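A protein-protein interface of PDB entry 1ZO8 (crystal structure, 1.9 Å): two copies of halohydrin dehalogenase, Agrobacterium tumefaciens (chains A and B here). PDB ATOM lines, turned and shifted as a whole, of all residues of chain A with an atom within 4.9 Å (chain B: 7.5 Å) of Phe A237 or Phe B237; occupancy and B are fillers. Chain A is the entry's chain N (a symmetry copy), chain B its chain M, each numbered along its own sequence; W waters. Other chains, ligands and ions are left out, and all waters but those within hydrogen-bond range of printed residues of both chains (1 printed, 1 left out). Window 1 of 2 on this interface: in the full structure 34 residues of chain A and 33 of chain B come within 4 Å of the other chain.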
ATOM      1  N   PHE A 171     -23.633  -4.639  28.655  1.00  0.00           N
ATOM      2  CA  PHE A 171     -22.972  -5.867  29.092  1.00  0.00           C
ATOM      3  C   PHE A 171     -21.610  -5.616  29.730  1.00  0.00           C
ATOM      4  O   PHE A 171     -20.972  -4.590  29.492  1.00  0.00           O
ATOM      5  CB  PHE A 171     -22.702  -6.812  27.912  1.00  0.00           C
ATOM      6  CG  PHE A 171     -23.827  -6.914  26.916  1.00  0.00           C
ATOM      7  CD1 PHE A 171     -23.835  -6.123  25.773  1.00  0.00           C
ATOM      8  CD2 PHE A 171     -24.855  -7.826  27.107  1.00  0.00           C
ATOM      9  CE1 PHE A 171     -24.852  -6.242  24.828  1.00  0.00           C
ATOM     10  CE2 PHE A 171     -25.882  -7.955  26.168  1.00  0.00           C
ATOM     11  CZ  PHE A 171     -25.877  -7.160  25.027  1.00  0.00           C
ATOM     12  N   ALA A 172     -21.159  -6.589  30.514  1.00  0.00           N
ATOM     13  CA  ALA A 172     -19.839  -6.532  31.129  1.00  0.00           C
ATOM     14  C   ALA A 172     -19.147  -7.859  30.814  1.00  0.00           C
ATOM     15  O   ALA A 172     -19.725  -8.929  31.013  1.00  0.00           O
ATOM     16  CB  ALA A 172     -19.951  -6.352  32.643  1.00  0.00           C
ATOM     17  N   ILE A 173     -17.924  -7.784  30.303  1.00  0.00           N
ATOM     18  CA  ILE A 173     -17.137  -8.975  29.996  1.00  0.00           C
ATOM     19  C   ILE A 173     -15.992  -8.952  30.997  1.00  0.00           C
ATOM     20  O   ILE A 173     -15.176  -8.032  30.971  1.00  0.00           O
ATOM     21  CB  ILE A 173     -16.520  -8.923  28.581  1.00  0.00           C
ATOM     22  CG1 ILE A 173     -17.618  -8.725  27.534  1.00  0.00           C
ATOM     23  CG2 ILE A 173     -15.734 -10.218  28.313  1.00  0.00           C
ATOM     24  CD1 ILE A 173     -18.702  -9.765  27.567  1.00  0.00           C
ATOM     25  N   GLY A 174     -15.951  -9.942  31.887  1.00  0.00           N
ATOM     26  CA  GLY A 174     -14.900 -10.013  32.892  1.00  0.00           C
ATOM     27  C   GLY A 174     -13.924 -11.115  32.549  1.00  0.00           C
ATOM     28  O   GLY A 174     -14.180 -12.287  32.822  1.00  0.00           O
ATOM     29  N   LEU A 220     -16.777 -12.273  20.958  1.00  0.00           N
ATOM     30  CA  LEU A 220     -17.844 -11.971  21.910  1.00  0.00           C
ATOM     31  C   LEU A 220     -18.271 -10.513  21.784  1.00  0.00           C
ATOM     32  O   LEU A 220     -19.462 -10.208  21.730  1.00  0.00           O
ATOM     33  CB  LEU A 220     -17.380 -12.268  23.347  1.00  0.00           C
ATOM     34  CG  LEU A 220     -18.413 -12.080  24.466  1.00  0.00           C
ATOM     35  CD1 LEU A 220     -19.646 -12.914  24.165  1.00  0.00           C
ATOM     36  CD2 LEU A 220     -17.817 -12.484  25.810  1.00  0.00           C
ATOM     37  N   LEU A 224     -22.027  -9.339  20.673  1.00  0.00           N
ATOM     38  CA  LEU A 224     -22.894  -8.547  21.539  1.00  0.00           C
ATOM     39  C   LEU A 224     -23.274  -7.212  20.919  1.00  0.00           C
ATOM     40  O   LEU A 224     -24.366  -6.704  21.158  1.00  0.00           O
ATOM     41  CB  LEU A 224     -22.219  -8.317  22.897  1.00  0.00           C
ATOM     42  CG  LEU A 224     -21.919  -9.595  23.684  1.00  0.00           C
ATOM     43  CD1 LEU A 224     -21.165  -9.247  24.957  1.00  0.00           C
ATOM     44  CD2 LEU A 224     -23.223 -10.326  24.004  1.00  0.00           C
ATOM     45  N   LEU A 232     -29.718 -10.407  26.197  1.00  0.00           N
ATOM     46  CA  LEU A 232     -28.762 -10.785  27.233  1.00  0.00           C
ATOM     47  C   LEU A 232     -28.390  -9.556  28.047  1.00  0.00           C
ATOM     48  O   LEU A 232     -27.561  -9.637  28.952  1.00  0.00           O
ATOM     49  CB  LEU A 232     -27.476 -11.359  26.614  1.00  0.00           C
ATOM     50  CG  LEU A 232     -27.519 -12.800  26.106  1.00  0.00           C
ATOM     51  CD1 LEU A 232     -26.215 -13.139  25.387  1.00  0.00           C
ATOM     52  CD2 LEU A 232     -27.753 -13.740  27.292  1.00  0.00           C
ATOM     53  N   GLN A 235     -26.106  -8.850  31.419  1.00  0.00           N
ATOM     54  CA  GLN A 235     -25.242  -9.996  31.670  1.00  0.00           C
ATOM     55  C   GLN A 235     -23.790  -9.652  31.954  1.00  0.00           C
ATOM     56  O   GLN A 235     -23.229  -8.744  31.344  1.00  0.00           O
ATOM     57  CB  GLN A 235     -25.263 -10.931  30.459  1.00  0.00           C
ATOM     58  CG  GLN A 235     -24.446 -12.206  30.628  1.00  0.00           C
ATOM     59  CD  GLN A 235     -25.150 -13.219  31.499  1.00  0.00           C
ATOM     60  OE1 GLN A 235     -26.310 -13.547  31.264  1.00  0.00           O
ATOM     61  NE2 GLN A 235     -24.452 -13.727  32.510  1.00  0.00           N
ATOM     62  N   VAL A 236     -23.194 -10.384  32.891  1.00  0.00           N
ATOM     63  CA  VAL A 236     -21.775 -10.246  33.181  1.00  0.00           C
ATOM     64  C   VAL A 236     -21.219 -11.570  32.650  1.00  0.00           C
ATOM     65  O   VAL A 236     -21.596 -12.647  33.125  1.00  0.00           O
ATOM     66  CB  VAL A 236     -21.475 -10.141  34.692  1.00  0.00           C
ATOM     67  CG1 VAL A 236     -19.965 -10.104  34.912  1.00  0.00           C
ATOM     68  CG2 VAL A 236     -22.110  -8.877  35.264  1.00  0.00           C
ATOM     69  N   PHE A 237     -20.357 -11.490  31.643  1.00  0.00           N
ATOM     70  CA  PHE A 237     -19.767 -12.681  31.034  1.00  0.00           C
ATOM     71  C   PHE A 237     -18.413 -13.004  31.658  1.00  0.00           C
ATOM     72  O   PHE A 237     -17.505 -12.182  31.624  1.00  0.00           O
ATOM     73  CB  PHE A 237     -19.581 -12.461  29.528  1.00  0.00           C
ATOM     74  CG  PHE A 237     -20.864 -12.192  28.775  1.00  0.00           C
ATOM     75  CD1 PHE A 237     -21.538 -13.223  28.130  1.00  0.00           C
ATOM     76  CD2 PHE A 237     -21.385 -10.903  28.693  1.00  0.00           C
ATOM     77  CE1 PHE A 237     -22.709 -12.976  27.413  1.00  0.00           C
ATOM     78  CE2 PHE A 237     -22.561 -10.640  27.975  1.00  0.00           C
ATOM     79  CZ  PHE A 237     -23.221 -11.676  27.336  1.00  0.00           C
ATOM     80  N   TRP A 238     -18.277 -14.195  32.235  1.00  0.00           N
ATOM     81  CA  TRP A 238     -17.001 -14.590  32.831  1.00  0.00           C
ATOM     82  C   TRP A 238     -16.162 -15.247  31.732  1.00  0.00           C
ATOM     83  O   TRP A 238     -16.340 -16.425  31.411  1.00  0.00           O
ATOM     84  CB  TRP A 238     -17.232 -15.559  33.993  1.00  0.00           C
ATOM     85  CG  TRP A 238     -18.106 -14.979  35.079  1.00  0.00           C
ATOM     86  CD1 TRP A 238     -19.283 -15.494  35.547  1.00  0.00           C
ATOM     87  CD2 TRP A 238     -17.879 -13.766  35.811  1.00  0.00           C
ATOM     88  NE1 TRP A 238     -19.804 -14.676  36.525  1.00  0.00           N
ATOM     89  CE2 TRP A 238     -18.962 -13.609  36.706  1.00  0.00           C
ATOM     90  CE3 TRP A 238     -16.866 -12.796  35.797  1.00  0.00           C
ATOM     91  CZ2 TRP A 238     -19.062 -12.518  37.583  1.00  0.00           C
ATOM     92  CZ3 TRP A 238     -16.965 -11.708  36.670  1.00  0.00           C
ATOM     93  CH2 TRP A 238     -18.059 -11.581  37.550  1.00  0.00           C
ATOM     94  N   LEU A 239     -15.257 -14.469  31.144  1.00  0.00           N
ATOM     95  CA  LEU A 239     -14.401 -14.960  30.061  1.00  0.00           C
ATOM     96  C   LEU A 239     -13.087 -15.415  30.673  1.00  0.00           C
ATOM     97  O   LEU A 239     -12.057 -14.758  30.507  1.00  0.00           O
ATOM     98  CB  LEU A 239     -14.129 -13.833  29.070  1.00  0.00           C
ATOM     99  CG  LEU A 239     -14.250 -14.041  27.557  1.00  0.00           C
ATOM    100  CD1 LEU A 239     -13.243 -13.120  26.893  1.00  0.00           C
ATOM    101  CD2 LEU A 239     -13.999 -15.474  27.151  1.00  0.00           C
ATOM    102  N   ILE B 128     -24.791 -27.605  25.503  1.00  0.00           N
ATOM    103  CA  ILE B 128     -25.621 -26.451  25.843  1.00  0.00           C
ATOM    104  C   ILE B 128     -26.937 -26.895  26.481  1.00  0.00           C
ATOM    105  O   ILE B 128     -27.702 -27.665  25.888  1.00  0.00           O
ATOM    106  CB  ILE B 128     -25.961 -25.602  24.592  1.00  0.00           C
ATOM    107  CG1 ILE B 128     -24.676 -25.110  23.919  1.00  0.00           C
ATOM    108  CG2 ILE B 128     -26.836 -24.411  24.989  1.00  0.00           C
ATOM    109  CD1 ILE B 128     -24.892 -24.513  22.530  1.00  0.00           C
ATOM    110  N   PHE B 129     -27.186 -26.422  27.699  1.00  0.00           N
ATOM    111  CA  PHE B 129     -28.430 -26.727  28.395  1.00  0.00           C
ATOM    112  C   PHE B 129     -29.317 -25.498  28.291  1.00  0.00           C
ATOM    113  O   PHE B 129     -28.849 -24.378  28.507  1.00  0.00           O
ATOM    114  CB  PHE B 129     -28.208 -26.983  29.890  1.00  0.00           C
ATOM    115  CG  PHE B 129     -27.522 -28.277  30.217  1.00  0.00           C
ATOM    116  CD1 PHE B 129     -27.279 -28.612  31.551  1.00  0.00           C
ATOM    117  CD2 PHE B 129     -27.108 -29.156  29.223  1.00  0.00           C
ATOM    118  CE1 PHE B 129     -26.635 -29.792  31.892  1.00  0.00           C
ATOM    119  CE2 PHE B 129     -26.460 -30.344  29.555  1.00  0.00           C
ATOM    120  CZ  PHE B 129     -26.224 -30.662  30.894  1.00  0.00           C
ATOM    121  N   THR B 131     -31.977 -23.947  30.180  1.00  0.00           N
ATOM    122  CA  THR B 131     -32.602 -24.068  31.484  1.00  0.00           C
ATOM    123  C   THR B 131     -33.681 -23.021  31.708  1.00  0.00           C
ATOM    124  O   THR B 131     -34.680 -22.990  30.997  1.00  0.00           O
ATOM    125  CB  THR B 131     -31.534 -23.969  32.595  1.00  0.00           C
ATOM    126  OG1 THR B 131     -30.843 -22.719  32.479  1.00  0.00           O
ATOM    127  CG2 THR B 131     -30.528 -25.107  32.467  1.00  0.00           C
ATOM    128  N   SER B 132     -33.479 -22.167  32.703  1.00  0.00           N
ATOM    129  CA  SER B 132     -34.451 -21.133  33.023  1.00  0.00           C
ATOM    130  C   SER B 132     -33.812 -20.026  33.844  1.00  0.00           C
ATOM    131  O   SER B 132     -32.829 -20.260  34.542  1.00  0.00           O
ATOM    132  CB  SER B 132     -35.606 -21.747  33.817  1.00  0.00           C
ATOM    133  OG  SER B 132     -36.428 -20.738  34.380  1.00  0.00           O
ATOM    134  N   ALA B 133     -34.373 -18.824  33.753  1.00  0.00           N
ATOM    135  CA  ALA B 133     -33.874 -17.688  34.516  1.00  0.00           C
ATOM    136  C   ALA B 133     -34.652 -17.531  35.830  1.00  0.00           C
ATOM    137  O   ALA B 133     -34.400 -16.599  36.595  1.00  0.00           O
ATOM    138  CB  ALA B 133     -33.984 -16.415  33.694  1.00  0.00           C
ATOM    139  N   CYS B 153     -28.668 -25.706  36.031  1.00  0.00           N
ATOM    140  CA  CYS B 153     -27.704 -24.628  35.796  1.00  0.00           C
ATOM    141  C   CYS B 153     -26.360 -24.969  36.422  1.00  0.00           C
ATOM    142  O   CYS B 153     -25.309 -24.792  35.800  1.00  0.00           O
ATOM    143  CB  CYS B 153     -28.212 -23.309  36.393  1.00  0.00           C
ATOM    144  SG  CYS B 153     -29.564 -22.539  35.488  1.00  0.00           S
ATOM    145  N   VAL B 170     -19.028 -26.118  28.057  1.00  0.00           N
ATOM    146  CA  VAL B 170     -20.375 -26.443  28.512  1.00  0.00           C
ATOM    147  C   VAL B 170     -21.035 -25.140  28.948  1.00  0.00           C
ATOM    148  O   VAL B 170     -20.447 -24.368  29.703  1.00  0.00           O
ATOM    149  CB  VAL B 170     -20.369 -27.394  29.729  1.00  0.00           C
ATOM    150  CG1 VAL B 170     -21.805 -27.797  30.058  1.00  0.00           C
ATOM    151  CG2 VAL B 170     -19.508 -28.619  29.450  1.00  0.00           C
ATOM    152  N   PHE B 171     -22.249 -24.902  28.471  1.00  0.00           N
ATOM    153  CA  PHE B 171     -22.968 -23.685  28.812  1.00  0.00           C
ATOM    154  C   PHE B 171     -24.402 -23.960  29.228  1.00  0.00           C
ATOM    155  O   PHE B 171     -24.964 -25.017  28.933  1.00  0.00           O
ATOM    156  CB  PHE B 171     -23.038 -22.729  27.618  1.00  0.00           C
ATOM    157  CG  PHE B 171     -21.743 -22.561  26.873  1.00  0.00           C
ATOM    158  CD1 PHE B 171     -21.498 -23.287  25.710  1.00  0.00           C
ATOM    159  CD2 PHE B 171     -20.793 -21.640  27.303  1.00  0.00           C
ATOM    160  CE1 PHE B 171     -20.321 -23.091  24.976  1.00  0.00           C
ATOM    161  CE2 PHE B 171     -19.613 -21.435  26.583  1.00  0.00           C
ATOM    162  CZ  PHE B 171     -19.377 -22.162  25.414  1.00  0.00           C
ATOM    163  N   ALA B 172     -24.993 -22.983  29.906  1.00  0.00           N
ATOM    164  CA  ALA B 172     -26.385 -23.060  30.309  1.00  0.00           C
ATOM    165  C   ALA B 172     -27.012 -21.738  29.902  1.00  0.00           C
ATOM    166  O   ALA B 172     -26.463 -20.671  30.193  1.00  0.00           O
ATOM    167  CB  ALA B 172     -26.504 -23.258  31.816  1.00  0.00           C
ATOM    168  N   ILE B 173     -28.128 -21.803  29.187  1.00  0.00           N
ATOM    169  CA  ILE B 173     -28.842 -20.600  28.781  1.00  0.00           C
ATOM    170  C   ILE B 173     -30.172 -20.663  29.520  1.00  0.00           C
ATOM    171  O   ILE B 173     -30.979 -21.562  29.280  1.00  0.00           O
ATOM    172  CB  ILE B 173     -29.123 -20.565  27.256  1.00  0.00           C
ATOM    173  CG1 ILE B 173     -27.804 -20.607  26.472  1.00  0.00           C
ATOM    174  CG2 ILE B 173     -29.911 -19.311  26.910  1.00  0.00           C
ATOM    175  CD1 ILE B 173     -27.985 -20.774  24.952  1.00  0.00           C
ATOM    176  N   GLY B 174     -30.385 -19.725  30.436  1.00  0.00           N
ATOM    177  CA  GLY B 174     -31.621 -19.706  31.203  1.00  0.00           C
ATOM    178  C   GLY B 174     -32.493 -18.562  30.741  1.00  0.00           C
ATOM    179  O   GLY B 174     -32.277 -17.414  31.130  1.00  0.00           O
ATOM    180  N   PRO B 175     -33.488 -18.836  29.891  1.00  0.00           N
ATOM    181  CA  PRO B 175     -34.334 -17.732  29.433  1.00  0.00           C
ATOM    182  C   PRO B 175     -35.570 -17.514  30.295  1.00  0.00           C
ATOM    183  O   PRO B 175     -35.865 -18.286  31.203  1.00  0.00           O
ATOM    184  CB  PRO B 175     -34.742 -18.162  28.015  1.00  0.00           C
ATOM    185  CG  PRO B 175     -33.997 -19.508  27.760  1.00  0.00           C
ATOM    186  CD  PRO B 175     -33.770 -20.062  29.132  1.00  0.00           C
ATOM    187  N   LEU B 220     -27.523 -17.099  19.890  1.00  0.00           N
ATOM    188  CA  LEU B 220     -26.616 -17.429  20.984  1.00  0.00           C
ATOM    189  C   LEU B 220     -26.166 -18.878  20.903  1.00  0.00           C
ATOM    190  O   LEU B 220     -24.987 -19.176  21.067  1.00  0.00           O
ATOM    191  CB  LEU B 220     -27.284 -17.167  22.336  1.00  0.00           C
ATOM    192  CG  LEU B 220     -26.511 -17.594  23.589  1.00  0.00           C
ATOM    193  CD1 LEU B 220     -25.105 -16.984  23.587  1.00  0.00           C
ATOM    194  CD2 LEU B 220     -27.288 -17.145  24.829  1.00  0.00           C
ATOM    195  N   PHE B 223     -23.742 -19.285  18.040  1.00  0.00           N
ATOM    196  CA  PHE B 223     -22.481 -18.642  18.400  1.00  0.00           C
ATOM    197  C   PHE B 223     -21.655 -19.538  19.315  1.00  0.00           C
ATOM    198  O   PHE B 223     -20.463 -19.748  19.078  1.00  0.00           O
ATOM    199  CB  PHE B 223     -22.757 -17.309  19.107  1.00  0.00           C
ATOM    200  CG  PHE B 223     -21.513 -16.592  19.565  1.00  0.00           C
ATOM    201  CD1 PHE B 223     -20.650 -16.017  18.643  1.00  0.00           C
ATOM    202  CD2 PHE B 223     -21.212 -16.488  20.921  1.00  0.00           C
ATOM    203  CE1 PHE B 223     -19.498 -15.342  19.065  1.00  0.00           C
ATOM    204  CE2 PHE B 223     -20.066 -15.816  21.351  1.00  0.00           C
ATOM    205  CZ  PHE B 223     -19.210 -15.242  20.415  1.00  0.00           C
ATOM    206  N   LEU B 224     -22.288 -20.056  20.366  1.00  0.00           N
ATOM    207  CA  LEU B 224     -21.609 -20.918  21.322  1.00  0.00           C
ATOM    208  C   LEU B 224     -21.144 -22.230  20.695  1.00  0.00           C
ATOM    209  O   LEU B 224     -20.049 -22.714  20.989  1.00  0.00           O
ATOM    210  CB  LEU B 224     -22.530 -21.212  22.513  1.00  0.00           C
ATOM    211  CG  LEU B 224     -22.883 -20.024  23.419  1.00  0.00           C
ATOM    212  CD1 LEU B 224     -23.947 -20.423  24.431  1.00  0.00           C
ATOM    213  CD2 LEU B 224     -21.626 -19.545  24.130  1.00  0.00           C
ATOM    214  N   CYS B 229     -16.115 -18.767  20.771  1.00  0.00           N
ATOM    215  CA  CYS B 229     -15.768 -18.275  22.095  1.00  0.00           C
ATOM    216  C   CYS B 229     -15.878 -19.357  23.163  1.00  0.00           C
ATOM    217  O   CYS B 229     -16.691 -19.250  24.079  1.00  0.00           O
ATOM    218  CB  CYS B 229     -16.677 -17.090  22.450  1.00  0.00           C
ATOM    219  SG  CYS B 229     -16.062 -16.045  23.782  1.00  0.00           S
ATOM    220  N   LEU B 232     -15.681 -19.034  27.238  1.00  0.00           N
ATOM    221  CA  LEU B 232     -16.816 -18.681  28.095  1.00  0.00           C
ATOM    222  C   LEU B 232     -17.337 -19.922  28.812  1.00  0.00           C
ATOM    223  O   LEU B 232     -18.346 -19.859  29.518  1.00  0.00           O
ATOM    224  CB  LEU B 232     -17.967 -18.094  27.273  1.00  0.00           C
ATOM    225  CG  LEU B 232     -17.932 -16.625  26.856  1.00  0.00           C
ATOM    226  CD1 LEU B 232     -19.144 -16.333  25.984  1.00  0.00           C
ATOM    227  CD2 LEU B 232     -17.925 -15.739  28.085  1.00  0.00           C
ATOM    228  N   THR B 233     -16.656 -21.052  28.641  1.00  0.00           N
ATOM    229  CA  THR B 233     -17.122 -22.291  29.261  1.00  0.00           C
ATOM    230  C   THR B 233     -17.485 -22.157  30.741  1.00  0.00           C
ATOM    231  O   THR B 233     -16.770 -21.513  31.513  1.00  0.00           O
ATOM    232  CB  THR B 233     -16.096 -23.434  29.102  1.00  0.00           C
ATOM    233  OG1 THR B 233     -16.708 -24.659  29.522  1.00  0.00           O
ATOM    234  CG2 THR B 233     -14.853 -23.186  29.962  1.00  0.00           C
ATOM    235  N   GLY B 234     -18.612 -22.763  31.118  1.00  0.00           N
ATOM    236  CA  GLY B 234     -19.081 -22.717  32.496  1.00  0.00           C
ATOM    237  C   GLY B 234     -20.085 -21.599  32.736  1.00  0.00           C
ATOM    238  O   GLY B 234     -20.723 -21.532  33.782  1.00  0.00           O
ATOM    239  N   GLN B 235     -20.230 -20.727  31.748  1.00  0.00           N
ATOM    240  CA  GLN B 235     -21.145 -19.592  31.828  1.00  0.00           C
ATOM    241  C   GLN B 235     -22.624 -19.960  31.824  1.00  0.00           C
ATOM    242  O   GLN B 235     -23.054 -20.847  31.086  1.00  0.00           O
ATOM    243  CB  GLN B 235     -20.917 -18.652  30.644  1.00  0.00           C
ATOM    244  CG  GLN B 235     -21.786 -17.397  30.675  1.00  0.00           C
ATOM    245  CD  GLN B 235     -21.260 -16.379  31.656  1.00  0.00           C
ATOM    246  OE1 GLN B 235     -20.082 -16.045  31.627  1.00  0.00           O
ATOM    247  NE2 GLN B 235     -22.129 -15.874  32.528  1.00  0.00           N
ATOM    248  N   VAL B 236     -23.388 -19.267  32.664  1.00  0.00           N
ATOM    249  CA  VAL B 236     -24.834 -19.425  32.713  1.00  0.00           C
ATOM    250  C   VAL B 236     -25.301 -18.085  32.155  1.00  0.00           C
ATOM    251  O   VAL B 236     -24.999 -17.022  32.718  1.00  0.00           O
ATOM    252  CB  VAL B 236     -25.377 -19.584  34.149  1.00  0.00           C
ATOM    253  CG1 VAL B 236     -26.905 -19.617  34.113  1.00  0.00           C
ATOM    254  CG2 VAL B 236     -24.851 -20.869  34.767  1.00  0.00           C
ATOM    255  N   PHE B 237     -26.005 -18.129  31.035  1.00  0.00           N
ATOM    256  CA  PHE B 237     -26.491 -16.921  30.380  1.00  0.00           C
ATOM    257  C   PHE B 237     -27.930 -16.650  30.775  1.00  0.00           C
ATOM    258  O   PHE B 237     -28.789 -17.513  30.601  1.00  0.00           O
ATOM    259  CB  PHE B 237     -26.452 -17.094  28.859  1.00  0.00           C
ATOM    260  CG  PHE B 237     -25.084 -17.339  28.299  1.00  0.00           C
ATOM    261  CD1 PHE B 237     -24.335 -16.291  27.769  1.00  0.00           C
ATOM    262  CD2 PHE B 237     -24.552 -18.621  28.278  1.00  0.00           C
ATOM    263  CE1 PHE B 237     -23.073 -16.521  27.223  1.00  0.00           C
ATOM    264  CE2 PHE B 237     -23.290 -18.863  27.734  1.00  0.00           C
ATOM    265  CZ  PHE B 237     -22.551 -17.814  27.207  1.00  0.00           C
ATOM    266  N   TRP B 238     -28.200 -15.463  31.305  1.00  0.00           N
ATOM    267  CA  TRP B 238     -29.564 -15.116  31.665  1.00  0.00           C
ATOM    268  C   TRP B 238     -30.164 -14.379  30.469  1.00  0.00           C
ATOM    269  O   TRP B 238     -29.922 -13.184  30.262  1.00  0.00           O
ATOM    270  CB  TRP B 238     -29.585 -14.233  32.912  1.00  0.00           C
ATOM    271  CG  TRP B 238     -28.902 -14.860  34.099  1.00  0.00           C
ATOM    272  CD1 TRP B 238     -27.844 -14.346  34.788  1.00  0.00           C
ATOM    273  CD2 TRP B 238     -29.252 -16.088  34.759  1.00  0.00           C
ATOM    274  NE1 TRP B 238     -27.513 -15.171  35.838  1.00  0.00           N
ATOM    275  CE2 TRP B 238     -28.361 -16.246  35.846  1.00  0.00           C
ATOM    276  CE3 TRP B 238     -30.232 -17.068  34.541  1.00  0.00           C
ATOM    277  CZ2 TRP B 238     -28.421 -17.342  36.715  1.00  0.00           C
ATOM    278  CZ3 TRP B 238     -30.290 -18.164  35.408  1.00  0.00           C
ATOM    279  CH2 TRP B 238     -29.388 -18.287  36.481  1.00  0.00           C
ATOM    280  N   LEU B 239     -30.923 -15.123  29.669  1.00  0.00           N
ATOM    281  CA  LEU B 239     -31.574 -14.597  28.476  1.00  0.00           C
ATOM    282  C   LEU B 239     -32.967 -14.151  28.902  1.00  0.00           C
ATOM    283  O   LEU B 239     -33.948 -14.813  28.579  1.00  0.00           O
ATOM    284  CB  LEU B 239     -31.705 -15.713  27.427  1.00  0.00           C
ATOM    285  CG  LEU B 239     -31.197 -15.573  25.985  1.00  0.00           C
ATOM    286  CD1 LEU B 239     -31.976 -16.565  25.121  1.00  0.00           C
ATOM    287  CD2 LEU B 239     -31.379 -14.166  25.456  1.00  0.00           C
ATOM    288  N   ALA B 240     -33.060 -13.035  29.619  1.00  0.00           N
ATOM    289  CA  ALA B 240     -34.361 -12.581  30.094  1.00  0.00           C
ATOM    290  C   ALA B 240     -34.620 -11.091  29.919  1.00  0.00           C
ATOM    291  O   ALA B 240     -35.457 -10.512  30.612  1.00  0.00           O
ATOM    292  CB  ALA B 240     -34.538 -12.985  31.560  1.00  0.00           C
HETATM  293  O   HOH W   1     -29.154 -10.791  31.544  1.00  0.00           O
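The backbone NH (N) of Trp B238 sits at hydrogen-bond distance from the side-chain amide oxygen (OE1) of Gln A235 (2.7 Å). The backbone carbonyl oxygen (O) of Val B236 lies within hydrogen-bond range of the side-chain amide nitrogen (NE2) of Gln A235 (3.3 Å). O of Val A236 lies within hydrogen-bond range of NE2 of Gln B235 (3.3 Å). OE1 of Gln B235 sits at hydrogen-bond distance from N of Trp A238, 2.7 Å away. The side-chain amide nitrogen (NE2) of Gln B235 sits close to the side-chain amide nitrogen (NE2) of Gln A235 (3.2 Å).
N of Phe B237 sits at hydrogen-bond distance from O of Ala B172, at 2.7 Å. N of Gly A174 lies within hydrogen-bond range of O of Phe A237 (2.7 Å). The backbone NH (N) of Ala A172 sits at hydrogen-bond distance from the backbone carbonyl oxygen (O) of Gln A235 (3.1 Å). N of Ala B172 sits at hydrogen-bond distance from O of Gln B235, at 3.1 Å. N of Gly B174 is in hydrogen-bond range of O of Phe B237, 2.7 Å away. The backbone carbonyl oxygen (O) of Ala A172 lies within hydrogen-bond range of the backbone NH (N) of Phe A237 (2.7 Å).
Leu A220 touches Phe B223. Leu A220 touches Leu B232 (CD1 to CD1, 3.9 Å). CD2 of Leu A232 touches CB of Phe B237, at 3.9 Å. Trp B238 touches Leu A232. Gln A235 touches Phe B237 (OE1 to CA, 3.5 Å). OE1 of Gln B235 touches CA of Phe A237, 3.4 Å away. CE1 of Phe A237 touches CE1 of Phe B237, 3.6 Å away. CD2 of Leu B232 touches O of Trp A238 (3.7 Å). Leu A239 touches Cys B229 (CD2 to SG, 3.99 Å). Leu A239 touches Leu B232.
Of the printed residues of chain B, Leu A220 touches Phe B223 (3.8 Å) and Leu B232 (3.9 Å). Printed residues of chain B within 4 Å of Val A236: Gln B235. Phe A237 touches just these residues of chain B: Leu B232 (3.9 Å), Gln B235 (3.4 Å) and Phe B237 (3.6 Å). Phe B129 touches none of the printed residues of chain A. Ala B172 touches none of the printed residues of chain A. Printed residues of chain A within 4 Å of Leu B232: Leu A220, Phe A237, Trp A238 and Leu A239. Printed residues of chain A within 4 Å of Gln B235: Gln A235 (3.2 Å), Val A236 (3.3 Å), Phe A237 (3.4 Å) and Trp A238 (2.7 Å). Of chain A, only Leu A232 (3.9 Å), Gln A235 (3.5 Å) and Phe A237 (3.6 Å) come within 4 Å of Phe B237. The nearest printed residue of chain A that does not touch Leu B232 is Ile A173 (5.9 Å).
Of the 12 printed residues of chain A, 7 touch a printed residue of chain B. Hydrophobic or aromatic side chains of chain A within 4 Å of the printed part of chain B: Leu A220, Leu A232, Phe A237, Trp A238 and Leu A239. Of the 25 printed residues of chain B, 7 touch a printed residue of chain A. Hydrophobic or aromatic side chains of chain B within 4 Å of the printed part of chain A: Phe B223, Leu B232, Phe B237 and Trp B238.
Leu A232 touches Phe B237, and with the chains exchanged Phe A237 touches Leu B232. Gln A235 touches Val B236, and with the chains exchanged Val A236 touches Gln B235. Gln A235 touches Phe B237, and with the chains exchanged Phe A237 touches Gln B235. Leu A239 touches Leu B232, but with the chains exchanged Leu A232 does not touch Leu B239 (4.1 Å). Of the 16 pairs that touch across the chains among the printed residues, 12 have their exchanged pair printed and touching as well.
Water W1 bridges the backbone carbonyl oxygen of Trp B238 (2.8 Å) and the backbone carbonyl oxygen of Leu A232 (3.3 Å).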
